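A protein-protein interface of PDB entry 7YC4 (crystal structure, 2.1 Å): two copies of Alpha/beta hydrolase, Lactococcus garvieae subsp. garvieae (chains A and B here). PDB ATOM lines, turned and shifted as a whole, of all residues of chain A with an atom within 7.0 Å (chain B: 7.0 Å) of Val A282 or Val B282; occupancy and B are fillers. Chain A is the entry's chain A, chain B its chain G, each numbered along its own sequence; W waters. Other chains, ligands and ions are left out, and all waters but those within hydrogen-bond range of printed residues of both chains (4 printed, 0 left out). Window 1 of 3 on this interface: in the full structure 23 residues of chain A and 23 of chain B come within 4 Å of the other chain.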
ATOM      1  N   LEU A 252     -31.214  32.508  12.600  1.00  0.00           N
ATOM      2  CA  LEU A 252     -30.708  31.131  12.771  1.00  0.00           C
ATOM      3  C   LEU A 252     -31.792  30.166  12.283  1.00  0.00           C
ATOM      4  O   LEU A 252     -32.922  30.222  12.784  1.00  0.00           O
ATOM      5  CB  LEU A 252     -30.323  30.928  14.235  1.00  0.00           C
ATOM      6  CG  LEU A 252     -29.888  29.533  14.655  1.00  0.00           C
ATOM      7  CD1 LEU A 252     -28.592  29.076  13.986  1.00  0.00           C
ATOM      8  CD2 LEU A 252     -29.788  29.492  16.174  1.00  0.00           C
ATOM      9  N   ILE A 253     -31.481  29.370  11.269  1.00  0.00           N
ATOM     10  CA  ILE A 253     -32.430  28.392  10.681  1.00  0.00           C
ATOM     11  C   ILE A 253     -31.841  27.008  10.879  1.00  0.00           C
ATOM     12  O   ILE A 253     -30.800  26.766  10.326  1.00  0.00           O
ATOM     13  CB  ILE A 253     -32.688  28.714   9.199  1.00  0.00           C
ATOM     14  CG1 ILE A 253     -33.429  30.047   9.072  1.00  0.00           C
ATOM     15  CG2 ILE A 253     -33.425  27.571   8.524  1.00  0.00           C
ATOM     16  CD1 ILE A 253     -33.695  30.470   7.652  1.00  0.00           C
ATOM     17  N   ILE A 254     -32.498  26.160  11.666  1.00  0.00           N
ATOM     18  CA  ILE A 254     -31.999  24.795  12.000  1.00  0.00           C
ATOM     19  C   ILE A 254     -32.871  23.776  11.260  1.00  0.00           C
ATOM     20  O   ILE A 254     -34.077  23.860  11.396  1.00  0.00           O
ATOM     21  CB  ILE A 254     -32.014  24.632  13.538  1.00  0.00           C
ATOM     22  CG1 ILE A 254     -30.848  25.398  14.184  1.00  0.00           C
ATOM     23  CG2 ILE A 254     -32.039  23.163  13.950  1.00  0.00           C
ATOM     24  CD1 ILE A 254     -31.057  25.722  15.650  1.00  0.00           C
ATOM     25  N   THR A 255     -32.278  22.846  10.520  1.00  0.00           N
ATOM     26  CA  THR A 255     -33.010  21.756   9.819  1.00  0.00           C
ATOM     27  C   THR A 255     -32.478  20.415  10.309  1.00  0.00           C
ATOM     28  O   THR A 255     -31.318  20.363  10.750  1.00  0.00           O
ATOM     29  CB  THR A 255     -32.891  21.878   8.294  1.00  0.00           C
ATOM     30  OG1 THR A 255     -31.511  21.812   7.930  1.00  0.00           O
ATOM     31  CG2 THR A 255     -33.507  23.166   7.800  1.00  0.00           C
ATOM     32  N   GLY A 256     -33.335  19.404  10.293  1.00  0.00           N
ATOM     33  CA  GLY A 256     -32.956  17.987  10.456  1.00  0.00           C
ATOM     34  C   GLY A 256     -32.918  17.319   9.104  1.00  0.00           C
ATOM     35  O   GLY A 256     -33.669  17.726   8.232  1.00  0.00           O
ATOM     36  N   GLU A 266     -34.150  25.106   4.070  1.00  0.00           N
ATOM     37  CA  GLU A 266     -32.801  25.369   3.510  1.00  0.00           C
ATOM     38  C   GLU A 266     -32.894  26.328   2.316  1.00  0.00           C
ATOM     39  O   GLU A 266     -31.939  27.063   2.102  1.00  0.00           O
ATOM     40  CB  GLU A 266     -32.132  24.038   3.202  1.00  0.00           C
ATOM     41  CG  GLU A 266     -31.606  23.369   4.462  1.00  0.00           C
ATOM     42  CD  GLU A 266     -31.170  21.930   4.320  1.00  0.00           C
ATOM     43  OE1 GLU A 266     -30.944  21.513   3.182  1.00  0.00           O
ATOM     44  OE2 GLU A 266     -31.008  21.236   5.373  1.00  0.00           O
ATOM     45  N   ALA A 269     -33.524  29.869   3.858  1.00  0.00           N
ATOM     46  CA  ALA A 269     -32.183  30.380   4.269  1.00  0.00           C
ATOM     47  C   ALA A 269     -31.476  31.040   3.054  1.00  0.00           C
ATOM     48  O   ALA A 269     -30.935  32.150   3.214  1.00  0.00           O
ATOM     49  CB  ALA A 269     -31.363  29.258   4.860  1.00  0.00           C
ATOM     50  N   THR A 280     -27.467  32.168   9.564  1.00  0.00           N
ATOM     51  CA  THR A 280     -26.744  30.933   9.978  1.00  0.00           C
ATOM     52  C   THR A 280     -27.682  29.757   9.712  1.00  0.00           C
ATOM     53  O   THR A 280     -28.679  29.675  10.411  1.00  0.00           O
ATOM     54  CB  THR A 280     -26.311  31.004  11.451  1.00  0.00           C
ATOM     55  OG1 THR A 280     -25.463  32.139  11.596  1.00  0.00           O
ATOM     56  CG2 THR A 280     -25.595  29.756  11.913  1.00  0.00           C
ATOM     57  N   GLN A 281     -27.373  28.901   8.743  1.00  0.00           N
ATOM     58  CA  GLN A 281     -28.195  27.720   8.388  1.00  0.00           C
ATOM     59  C   GLN A 281     -27.373  26.474   8.680  1.00  0.00           C
ATOM     60  O   GLN A 281     -26.229  26.396   8.219  1.00  0.00           O
ATOM     61  CB  GLN A 281     -28.676  27.723   6.939  1.00  0.00           C
ATOM     62  CG  GLN A 281     -29.920  26.868   6.724  1.00  0.00           C
ATOM     63  CD  GLN A 281     -29.708  25.380   6.864  1.00  0.00           C
ATOM     64  OE1 GLN A 281     -28.874  24.753   6.193  1.00  0.00           O
ATOM     65  NE2 GLN A 281     -30.487  24.783   7.748  1.00  0.00           N
ATOM     66  N   VAL A 282     -27.950  25.565   9.457  1.00  0.00           N
ATOM     67  CA  VAL A 282     -27.257  24.342   9.941  1.00  0.00           C
ATOM     68  C   VAL A 282     -28.248  23.190   9.905  1.00  0.00           C
ATOM     69  O   VAL A 282     -29.363  23.369  10.435  1.00  0.00           O
ATOM     70  CB  VAL A 282     -26.719  24.561  11.362  1.00  0.00           C
ATOM     71  CG1 VAL A 282     -26.365  23.247  12.000  1.00  0.00           C
ATOM     72  CG2 VAL A 282     -25.521  25.494  11.363  1.00  0.00           C
ATOM     73  N   ARG A 283     -27.822  22.077   9.308  1.00  0.00           N
ATOM     74  CA  ARG A 283     -28.596  20.828   9.213  1.00  0.00           C
ATOM     75  C   ARG A 283     -27.964  19.760  10.118  1.00  0.00           C
ATOM     76  O   ARG A 283     -26.776  19.418   9.915  1.00  0.00           O
ATOM     77  CB  ARG A 283     -28.584  20.312   7.781  1.00  0.00           C
ATOM     78  CG  ARG A 283     -29.415  19.054   7.634  1.00  0.00           C
ATOM     79  CD  ARG A 283     -28.914  18.208   6.511  1.00  0.00           C
ATOM     80  NE  ARG A 283     -29.438  18.726   5.271  1.00  0.00           N
ATOM     81  CZ  ARG A 283     -29.312  18.102   4.125  1.00  0.00           C
ATOM     82  NH1 ARG A 283     -28.633  16.976   4.074  1.00  0.00           N
ATOM     83  NH2 ARG A 283     -29.834  18.626   3.033  1.00  0.00           N
ATOM     84  N   PHE A 284     -28.755  19.189  11.015  1.00  0.00           N
ATOM     85  CA  PHE A 284     -28.323  18.085  11.911  1.00  0.00           C
ATOM     86  C   PHE A 284     -28.603  16.751  11.225  1.00  0.00           C
ATOM     87  O   PHE A 284     -29.727  16.526  10.730  1.00  0.00           O
ATOM     88  CB  PHE A 284     -28.990  18.257  13.274  1.00  0.00           C
ATOM     89  CG  PHE A 284     -28.523  19.498  13.989  1.00  0.00           C
ATOM     90  CD1 PHE A 284     -29.118  20.725  13.755  1.00  0.00           C
ATOM     91  CD2 PHE A 284     -27.443  19.448  14.852  1.00  0.00           C
ATOM     92  CE1 PHE A 284     -28.644  21.871  14.369  1.00  0.00           C
ATOM     93  CE2 PHE A 284     -26.978  20.595  15.481  1.00  0.00           C
ATOM     94  CZ  PHE A 284     -27.584  21.805  15.232  1.00  0.00           C
ATOM     95  N   GLN A 285     -27.606  15.882  11.195  1.00  0.00           N
ATOM     96  CA  GLN A 285     -27.722  14.532  10.605  1.00  0.00           C
ATOM     97  C   GLN A 285     -28.659  13.663  11.466  1.00  0.00           C
ATOM     98  O   GLN A 285     -28.774  13.870  12.685  1.00  0.00           O
ATOM     99  CB  GLN A 285     -26.352  13.883  10.448  1.00  0.00           C
ATOM    100  CG  GLN A 285     -26.345  12.738   9.438  1.00  0.00           C
ATOM    101  CD  GLN A 285     -25.013  12.041   9.348  1.00  0.00           C
ATOM    102  OE1 GLN A 285     -24.481  11.537  10.325  1.00  0.00           O
ATOM    103  NE2 GLN A 285     -24.448  12.011   8.154  1.00  0.00           N
ATOM    104  N   PHE A 291     -37.554  17.553  16.844  1.00  0.00           N
ATOM    105  CA  PHE A 291     -36.500  16.990  17.735  1.00  0.00           C
ATOM    106  C   PHE A 291     -36.178  17.876  18.950  1.00  0.00           C
ATOM    107  O   PHE A 291     -35.696  17.290  19.970  1.00  0.00           O
ATOM    108  CB  PHE A 291     -35.249  16.580  16.953  1.00  0.00           C
ATOM    109  CG  PHE A 291     -34.373  17.655  16.357  1.00  0.00           C
ATOM    110  CD1 PHE A 291     -34.690  18.249  15.148  1.00  0.00           C
ATOM    111  CD2 PHE A 291     -33.170  18.009  16.959  1.00  0.00           C
ATOM    112  CE1 PHE A 291     -33.836  19.174  14.562  1.00  0.00           C
ATOM    113  CE2 PHE A 291     -32.338  18.969  16.395  1.00  0.00           C
ATOM    114  CZ  PHE A 291     -32.674  19.552  15.198  1.00  0.00           C
ATOM    115  N   HIS A 301     -28.170  13.786  20.343  1.00  0.00           N
ATOM    116  CA  HIS A 301     -26.973  14.622  20.053  1.00  0.00           C
ATOM    117  C   HIS A 301     -27.409  15.843  19.255  1.00  0.00           C
ATOM    118  O   HIS A 301     -26.923  16.945  19.517  1.00  0.00           O
ATOM    119  CB  HIS A 301     -25.918  13.802  19.320  1.00  0.00           C
ATOM    120  CG  HIS A 301     -25.428  12.672  20.155  1.00  0.00           C
ATOM    121  ND1 HIS A 301     -24.791  12.884  21.362  1.00  0.00           N
ATOM    122  CD2 HIS A 301     -25.523  11.330  19.992  1.00  0.00           C
ATOM    123  CE1 HIS A 301     -24.500  11.714  21.902  1.00  0.00           C
ATOM    124  NE2 HIS A 301     -24.931  10.751  21.077  1.00  0.00           N
ATOM    125  N   ALA A 302     -28.344  15.648  18.332  1.00  0.00           N
ATOM    126  CA  ALA A 302     -28.897  16.738  17.510  1.00  0.00           C
ATOM    127  C   ALA A 302     -29.555  17.758  18.433  1.00  0.00           C
ATOM    128  O   ALA A 302     -29.264  18.927  18.286  1.00  0.00           O
ATOM    129  CB  ALA A 302     -29.861  16.204  16.477  1.00  0.00           C
ATOM    130  N   ALA A 305     -26.991  19.661  20.685  1.00  0.00           N
ATOM    131  CA  ALA A 305     -26.151  20.572  19.885  1.00  0.00           C
ATOM    132  C   ALA A 305     -27.026  21.722  19.358  1.00  0.00           C
ATOM    133  O   ALA A 305     -26.574  22.893  19.349  1.00  0.00           O
ATOM    134  CB  ALA A 305     -25.494  19.759  18.824  1.00  0.00           C
ATOM    135  N   ALA A 306     -28.273  21.438  18.982  1.00  0.00           N
ATOM    136  CA  ALA A 306     -29.199  22.473  18.449  1.00  0.00           C
ATOM    137  C   ALA A 306     -29.539  23.470  19.565  1.00  0.00           C
ATOM    138  O   ALA A 306     -29.521  24.714  19.284  1.00  0.00           O
ATOM    139  CB  ALA A 306     -30.433  21.859  17.832  1.00  0.00           C
ATOM    140  N   LEU A 309     -26.197  25.478  20.324  1.00  0.00           N
ATOM    141  CA  LEU A 309     -25.970  26.462  19.235  1.00  0.00           C
ATOM    142  C   LEU A 309     -27.011  27.584  19.292  1.00  0.00           C
ATOM    143  O   LEU A 309     -26.597  28.745  19.241  1.00  0.00           O
ATOM    144  CB  LEU A 309     -25.991  25.764  17.875  1.00  0.00           C
ATOM    145  CG  LEU A 309     -25.634  26.673  16.701  1.00  0.00           C
ATOM    146  CD1 LEU A 309     -24.135  26.928  16.671  1.00  0.00           C
ATOM    147  CD2 LEU A 309     -26.127  26.099  15.397  1.00  0.00           C
ATOM    148  N   LEU B 252     -17.464  14.588  17.050  1.00  0.00           N
ATOM    149  CA  LEU B 252     -18.091  15.745  16.397  1.00  0.00           C
ATOM    150  C   LEU B 252     -17.561  15.815  14.968  1.00  0.00           C
ATOM    151  O   LEU B 252     -16.333  15.911  14.778  1.00  0.00           O
ATOM    152  CB  LEU B 252     -17.813  17.043  17.166  1.00  0.00           C
ATOM    153  CG  LEU B 252     -18.410  18.301  16.524  1.00  0.00           C
ATOM    154  CD1 LEU B 252     -19.904  18.152  16.318  1.00  0.00           C
ATOM    155  CD2 LEU B 252     -18.135  19.541  17.360  1.00  0.00           C
ATOM    156  N   ILE B 253     -18.467  15.703  13.991  1.00  0.00           N
ATOM    157  CA  ILE B 253     -18.113  15.738  12.549  1.00  0.00           C
ATOM    158  C   ILE B 253     -18.847  16.899  11.890  1.00  0.00           C
ATOM    159  O   ILE B 253     -20.088  16.911  11.878  1.00  0.00           O
ATOM    160  CB  ILE B 253     -18.391  14.382  11.888  1.00  0.00           C
ATOM    161  CG1 ILE B 253     -17.565  13.282  12.567  1.00  0.00           C
ATOM    162  CG2 ILE B 253     -18.163  14.464  10.370  1.00  0.00           C
ATOM    163  CD1 ILE B 253     -17.813  11.870  12.044  1.00  0.00           C
ATOM    164  N   ILE B 254     -18.077  17.847  11.373  1.00  0.00           N
ATOM    165  CA  ILE B 254     -18.591  19.097  10.753  1.00  0.00           C
ATOM    166  C   ILE B 254     -18.328  18.984   9.243  1.00  0.00           C
ATOM    167  O   ILE B 254     -17.186  18.654   8.849  1.00  0.00           O
ATOM    168  CB  ILE B 254     -17.912  20.298  11.438  1.00  0.00           C
ATOM    169  CG1 ILE B 254     -18.401  20.460  12.881  1.00  0.00           C
ATOM    170  CG2 ILE B 254     -18.089  21.575  10.635  1.00  0.00           C
ATOM    171  CD1 ILE B 254     -17.663  21.528  13.665  1.00  0.00           C
ATOM    172  N   THR B 255     -19.365  19.158   8.422  1.00  0.00           N
ATOM    173  CA  THR B 255     -19.224  19.234   6.954  1.00  0.00           C
ATOM    174  C   THR B 255     -19.739  20.585   6.458  1.00  0.00           C
ATOM    175  O   THR B 255     -20.546  21.241   7.162  1.00  0.00           O
ATOM    176  CB  THR B 255     -19.928  18.070   6.254  1.00  0.00           C
ATOM    177  OG1 THR B 255     -21.285  18.099   6.714  1.00  0.00           O
ATOM    178  CG2 THR B 255     -19.244  16.733   6.459  1.00  0.00           C
ATOM    179  N   GLY B 256     -19.204  21.001   5.309  1.00  0.00           N
ATOM    180  CA  GLY B 256     -19.707  22.113   4.496  1.00  0.00           C
ATOM    181  C   GLY B 256     -20.574  21.600   3.361  1.00  0.00           C
ATOM    182  O   GLY B 256     -20.274  20.551   2.796  1.00  0.00           O
ATOM    183  N   GLU B 266     -20.088  12.753   5.954  1.00  0.00           N
ATOM    184  CA  GLU B 266     -21.440  12.399   6.438  1.00  0.00           C
ATOM    185  C   GLU B 266     -21.569  10.874   6.430  1.00  0.00           C
ATOM    186  O   GLU B 266     -22.125  10.354   7.393  1.00  0.00           O
ATOM    187  CB  GLU B 266     -22.495  13.157   5.642  1.00  0.00           C
ATOM    188  CG  GLU B 266     -22.532  14.630   6.046  1.00  0.00           C
ATOM    189  CD  GLU B 266     -23.258  15.555   5.089  1.00  0.00           C
ATOM    190  OE1 GLU B 266     -23.805  15.038   4.108  1.00  0.00           O
ATOM    191  OE2 GLU B 266     -23.248  16.787   5.309  1.00  0.00           O
ATOM    192  N   ALA B 269     -19.764   9.487   9.508  1.00  0.00           N
ATOM    193  CA  ALA B 269     -20.570   9.789  10.719  1.00  0.00           C
ATOM    194  C   ALA B 269     -21.597   8.665  10.924  1.00  0.00           C
ATOM    195  O   ALA B 269     -21.829   8.249  12.109  1.00  0.00           O
ATOM    196  CB  ALA B 269     -21.214  11.135  10.595  1.00  0.00           C
ATOM    197  N   THR B 280     -22.131  13.452  16.863  1.00  0.00           N
ATOM    198  CA  THR B 280     -22.795  14.730  16.547  1.00  0.00           C
ATOM    199  C   THR B 280     -22.297  15.141  15.157  1.00  0.00           C
ATOM    200  O   THR B 280     -21.058  15.323  14.987  1.00  0.00           O
ATOM    201  CB  THR B 280     -22.523  15.780  17.627  1.00  0.00           C
ATOM    202  OG1 THR B 280     -22.888  15.250  18.907  1.00  0.00           O
ATOM    203  CG2 THR B 280     -23.256  17.075  17.352  1.00  0.00           C
ATOM    204  N   GLN B 281     -23.202  15.190  14.180  1.00  0.00           N
ATOM    205  CA  GLN B 281     -22.839  15.492  12.775  1.00  0.00           C
ATOM    206  C   GLN B 281     -23.709  16.632  12.307  1.00  0.00           C
ATOM    207  O   GLN B 281     -24.938  16.531  12.472  1.00  0.00           O
ATOM    208  CB  GLN B 281     -22.986  14.282  11.838  1.00  0.00           C
ATOM    209  CG  GLN B 281     -22.229  14.445  10.525  1.00  0.00           C
ATOM    210  CD  GLN B 281     -22.723  15.535   9.605  1.00  0.00           C
ATOM    211  OE1 GLN B 281     -23.922  15.672   9.328  1.00  0.00           O
ATOM    212  NE2 GLN B 281     -21.785  16.340   9.107  1.00  0.00           N
ATOM    213  N   VAL B 282     -23.078  17.675  11.766  1.00  0.00           N
ATOM    214  CA  VAL B 282     -23.737  18.975  11.488  1.00  0.00           C
ATOM    215  C   VAL B 282     -23.155  19.484  10.169  1.00  0.00           C
ATOM    216  O   VAL B 282     -21.882  19.466   9.998  1.00  0.00           O
ATOM    217  CB  VAL B 282     -23.561  19.967  12.656  1.00  0.00           C
ATOM    218  CG1 VAL B 282     -24.212  21.302  12.386  1.00  0.00           C
ATOM    219  CG2 VAL B 282     -24.144  19.438  13.948  1.00  0.00           C
ATOM    220  N   ARG B 283     -24.045  19.821   9.231  1.00  0.00           N
ATOM    221  CA  ARG B 283     -23.647  20.359   7.909  1.00  0.00           C
ATOM    222  C   ARG B 283     -23.985  21.847   7.886  1.00  0.00           C
ATOM    223  O   ARG B 283     -25.166  22.197   8.134  1.00  0.00           O
ATOM    224  CB  ARG B 283     -24.351  19.659   6.744  1.00  0.00           C
ATOM    225  CG  ARG B 283     -23.948  20.225   5.386  1.00  0.00           C
ATOM    226  CD  ARG B 283     -24.974  20.006   4.298  1.00  0.00           C
ATOM    227  NE  ARG B 283     -25.013  18.593   3.974  1.00  0.00           N
ATOM    228  CZ  ARG B 283     -25.752  18.070   3.000  1.00  0.00           C
ATOM    229  NH1 ARG B 283     -26.510  18.854   2.272  1.00  0.00           N
ATOM    230  NH2 ARG B 283     -25.698  16.781   2.739  1.00  0.00           N
ATOM    231  N   PHE B 284     -22.994  22.673   7.578  1.00  0.00           N
ATOM    232  CA  PHE B 284     -23.144  24.148   7.482  1.00  0.00           C
ATOM    233  C   PHE B 284     -23.420  24.459   6.010  1.00  0.00           C
ATOM    234  O   PHE B 284     -22.732  23.891   5.164  1.00  0.00           O
ATOM    235  CB  PHE B 284     -21.921  24.864   8.078  1.00  0.00           C
ATOM    236  CG  PHE B 284     -21.768  24.650   9.561  1.00  0.00           C
ATOM    237  CD1 PHE B 284     -21.246  23.470  10.056  1.00  0.00           C
ATOM    238  CD2 PHE B 284     -22.254  25.584  10.462  1.00  0.00           C
ATOM    239  CE1 PHE B 284     -21.192  23.238  11.423  1.00  0.00           C
ATOM    240  CE2 PHE B 284     -22.189  25.360  11.827  1.00  0.00           C
ATOM    241  CZ  PHE B 284     -21.659  24.186  12.303  1.00  0.00           C
ATOM    242  N   GLN B 285     -24.451  25.271   5.751  1.00  0.00           N
ATOM    243  CA  GLN B 285     -24.930  25.664   4.396  1.00  0.00           C
ATOM    244  C   GLN B 285     -23.984  26.713   3.790  1.00  0.00           C
ATOM    245  O   GLN B 285     -23.361  27.502   4.526  1.00  0.00           O
ATOM    246  CB  GLN B 285     -26.333  26.288   4.455  1.00  0.00           C
ATOM    247  CG  GLN B 285     -27.048  26.246   3.110  1.00  0.00           C
ATOM    248  CD  GLN B 285     -28.393  26.923   3.124  1.00  0.00           C
ATOM    249  OE1 GLN B 285     -28.544  28.072   3.543  1.00  0.00           O
ATOM    250  NE2 GLN B 285     -29.386  26.203   2.640  1.00  0.00           N
ATOM    251  N   PHE B 291     -13.109  26.097   5.656  1.00  0.00           N
ATOM    252  CA  PHE B 291     -13.798  27.336   6.085  1.00  0.00           C
ATOM    253  C   PHE B 291     -13.432  27.745   7.526  1.00  0.00           C
ATOM    254  O   PHE B 291     -13.528  28.953   7.844  1.00  0.00           O
ATOM    255  CB  PHE B 291     -15.299  27.190   5.826  1.00  0.00           C
ATOM    256  CG  PHE B 291     -16.079  26.310   6.763  1.00  0.00           C
ATOM    257  CD1 PHE B 291     -16.298  24.976   6.474  1.00  0.00           C
ATOM    258  CD2 PHE B 291     -16.712  26.858   7.862  1.00  0.00           C
ATOM    259  CE1 PHE B 291     -17.107  24.190   7.282  1.00  0.00           C
ATOM    260  CE2 PHE B 291     -17.503  26.065   8.686  1.00  0.00           C
ATOM    261  CZ  PHE B 291     -17.682  24.733   8.412  1.00  0.00           C
ATOM    262  N   HIS B 301     -20.792  33.277   8.780  1.00  0.00           N
ATOM    263  CA  HIS B 301     -21.793  32.710   9.716  1.00  0.00           C
ATOM    264  C   HIS B 301     -21.448  31.246   9.933  1.00  0.00           C
ATOM    265  O   HIS B 301     -21.455  30.850  11.099  1.00  0.00           O
ATOM    266  CB  HIS B 301     -23.204  32.958   9.194  1.00  0.00           C
ATOM    267  CG  HIS B 301     -23.422  34.411   9.044  1.00  0.00           C
ATOM    268  ND1 HIS B 301     -23.507  35.240  10.135  1.00  0.00           N
ATOM    269  CD2 HIS B 301     -23.535  35.193   7.944  1.00  0.00           C
ATOM    270  CE1 HIS B 301     -23.668  36.486   9.721  1.00  0.00           C
ATOM    271  NE2 HIS B 301     -23.704  36.480   8.379  1.00  0.00           N
ATOM    272  N   ALA B 302     -21.086  30.501   8.886  1.00  0.00           N
ATOM    273  CA  ALA B 302     -20.654  29.093   9.026  1.00  0.00           C
ATOM    274  C   ALA B 302     -19.432  28.986   9.962  1.00  0.00           C
ATOM    275  O   ALA B 302     -19.461  28.116  10.874  1.00  0.00           O
ATOM    276  CB  ALA B 302     -20.349  28.445   7.712  1.00  0.00           C
ATOM    277  N   ALA B 305     -20.466  29.822  13.596  1.00  0.00           N
ATOM    278  CA  ALA B 305     -21.363  28.797  14.181  1.00  0.00           C
ATOM    279  C   ALA B 305     -20.556  27.509  14.408  1.00  0.00           C
ATOM    280  O   ALA B 305     -20.730  26.859  15.450  1.00  0.00           O
ATOM    281  CB  ALA B 305     -22.599  28.638  13.309  1.00  0.00           C
ATOM    282  N   ALA B 306     -19.643  27.146  13.514  1.00  0.00           N
ATOM    283  CA  ALA B 306     -18.853  25.892  13.627  1.00  0.00           C
ATOM    284  C   ALA B 306     -17.855  26.005  14.786  1.00  0.00           C
ATOM    285  O   ALA B 306     -17.611  25.010  15.503  1.00  0.00           O
ATOM    286  CB  ALA B 306     -18.158  25.572  12.335  1.00  0.00           C
ATOM    287  N   LEU B 309     -20.059  25.851  18.034  1.00  0.00           N
ATOM    288  CA  LEU B 309     -20.559  24.468  18.263  1.00  0.00           C
ATOM    289  C   LEU B 309     -19.405  23.564  18.729  1.00  0.00           C
ATOM    290  O   LEU B 309     -19.611  22.792  19.660  1.00  0.00           O
ATOM    291  CB  LEU B 309     -21.200  23.903  16.990  1.00  0.00           C
ATOM    292  CG  LEU B 309     -21.401  22.388  17.014  1.00  0.00           C
ATOM    293  CD1 LEU B 309     -22.510  22.034  17.976  1.00  0.00           C
ATOM    294  CD2 LEU B 309     -21.662  21.813  15.629  1.00  0.00           C
HETATM  295  O   HOH W   1     -27.040  23.057   5.755  1.00  0.00           O
HETATM  296  O   HOH W   2     -24.501  16.989  20.534  1.00  0.00           O
HETATM  297  O   HOH W   3     -26.185  16.851   8.422  1.00  0.00           O
HETATM  298  O   HOH W   4     -23.231  32.118  12.936  1.00  0.00           O
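The backbone carbonyl oxygen (O) of Ile A253 lies within hydrogen-bond range of the side-chain amide nitrogen (NE2) of Gln A281 (3.3 Å).
O of Ile A253 sits at hydrogen-bond distance from N of Val A282 (3.2 Å).
The side-chain carboxylate of Glu B266 lies within hydrogen-bond range of the side-chain hydroxyl of Thr B255 (2.7 Å).
The guanidinium group of Arg B283 is in salt-bridge range of the side-chain carboxylate of Glu B266, at 2.9 Å.
Of the 19 printed residues of chain B, 11 touch a printed residue of chain A.
Hydrophobic or aromatic side chains of chain B that line the printed part of chain A: Ala B269, Val B282, Phe B284, His B301, Ala B305 and Leu B309.
Printed residues of chain A that touch a printed residue of chain B: Glu A266, Ala A269, Thr A280, Gln A281, Val A282, Arg A283, Phe A284, Gln A285, His A301, Ala A305 and Leu A309.
Hydrophobic or aromatic side chains of chain A within 4 Å of the printed part of chain B: Ala A269, Val A282, Phe A284, His A301, Ala A305 and Leu A309.
Among the printed residues, 20 pairs touch across the chains.
Of the printed residues of chain B, Ala A269 touches Gln B285.
Val A282 touches just these residues of chain B: Val B282 (2.9 Å), Arg B283 (3.5 Å) and Phe B284 (3.4 Å).
Printed residues of chain B within 4 Å of Phe A284: Gln B281 (3.8 Å) and Val B282 (3.4 Å).
Printed residues of chain B within 4 Å of Leu A309: Ala B305 (3.6 Å).
Ile B254 touches none of the printed residues of chain A.
Gly B256 touches none of the printed residues of chain A.
Val B282 touches just these residues of chain A: Val A282 (2.9 Å), Arg A283 (3.5 Å) and Phe A284 (3.4 Å).
Of the printed residues of chain A, His B301 touches Thr A280.
The nearest residue of chain B that does not touch Val A282 is Ala B305 (4.7 Å).
The nearest residue of chain A that does not touch Val B282 is Gln A285 (4.9 Å).
Glu A266 touches Gln B285, and with the chains exchanged Gln A285 touches Glu B266.
Ala A269 touches Gln B285, and with the chains exchanged Gln A285 touches Ala B269.
Thr A280 touches Ala B305, and with the chains exchanged Ala A305 touches Thr B280.
Val A282 touches Arg B283, and with the chains exchanged Arg A283 touches Val B282.
Of the 20 pairs that touch across the chains among the printed residues, 20 have their exchanged pair printed and touching as well.
Water W1 lies within hydrogen-bond range of the side-chain amide oxygen (OE1) of Gln A281 (2.5 Å), the backbone carbonyl oxygen (O) of Arg B283 (3.1 Å) and the backbone NH (N) of Gln B285 (3.4 Å).
Water W4 bridges OG1 of Thr A280 (2.6 Å) and O of His B301 (2.9 Å).
Water W3 lies within hydrogen-bond range of the side-chain amide oxygen (OE1) of Gln B281 (2.7 Å), the backbone carbonyl oxygen (O) of Arg A283 (3.0 Å) and the backbone NH (N) of Gln A285 (3.3 Å).
OE1 of Gln B285 touches CB of Ala A269, 3.3 Å away.
O of Gln A281 touches CA of Phe B284 (3.9 Å).
CG1 of Val A282 touches CG1 of Val B282, at 2.9 Å.
Arg B283 touches Val A282 (O to CA, 3.5 Å).
Gln B281 touches Phe A284.
Val B282 touches Phe A284 (CG2 to CD2, 3.4 Å).
OG1 of Thr B280 touches CB of His A301, 3.4 Å away.
CG2 of Thr B280 touches CB of Ala A305, 3.8 Å away.
Ala A305 touches Leu B309.
Leu A309 touches Ala B305.
The side-chain amide nitrogen (NE2) of Gln B285 lies within hydrogen-bond range of the backbone carbonyl oxygen (O) of Glu A266, 2.7 Å away.
The backbone NH (N) of Gln B285 sits at hydrogen-bond distance from the backbone carbonyl oxygen (O) of Gln A281.
The backbone carbonyl oxygen (O) of Arg A283 lies within hydrogen-bond range of the backbone NH (N) of Arg B283 (2.8 Å).
The backbone carbonyl oxygen (O) of Glu B266 sits at hydrogen-bond distance from the side-chain amide nitrogen (NE2) of Gln A285.
O of Gln B281 is in hydrogen-bond range of N of Gln A285 (3.0 Å).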
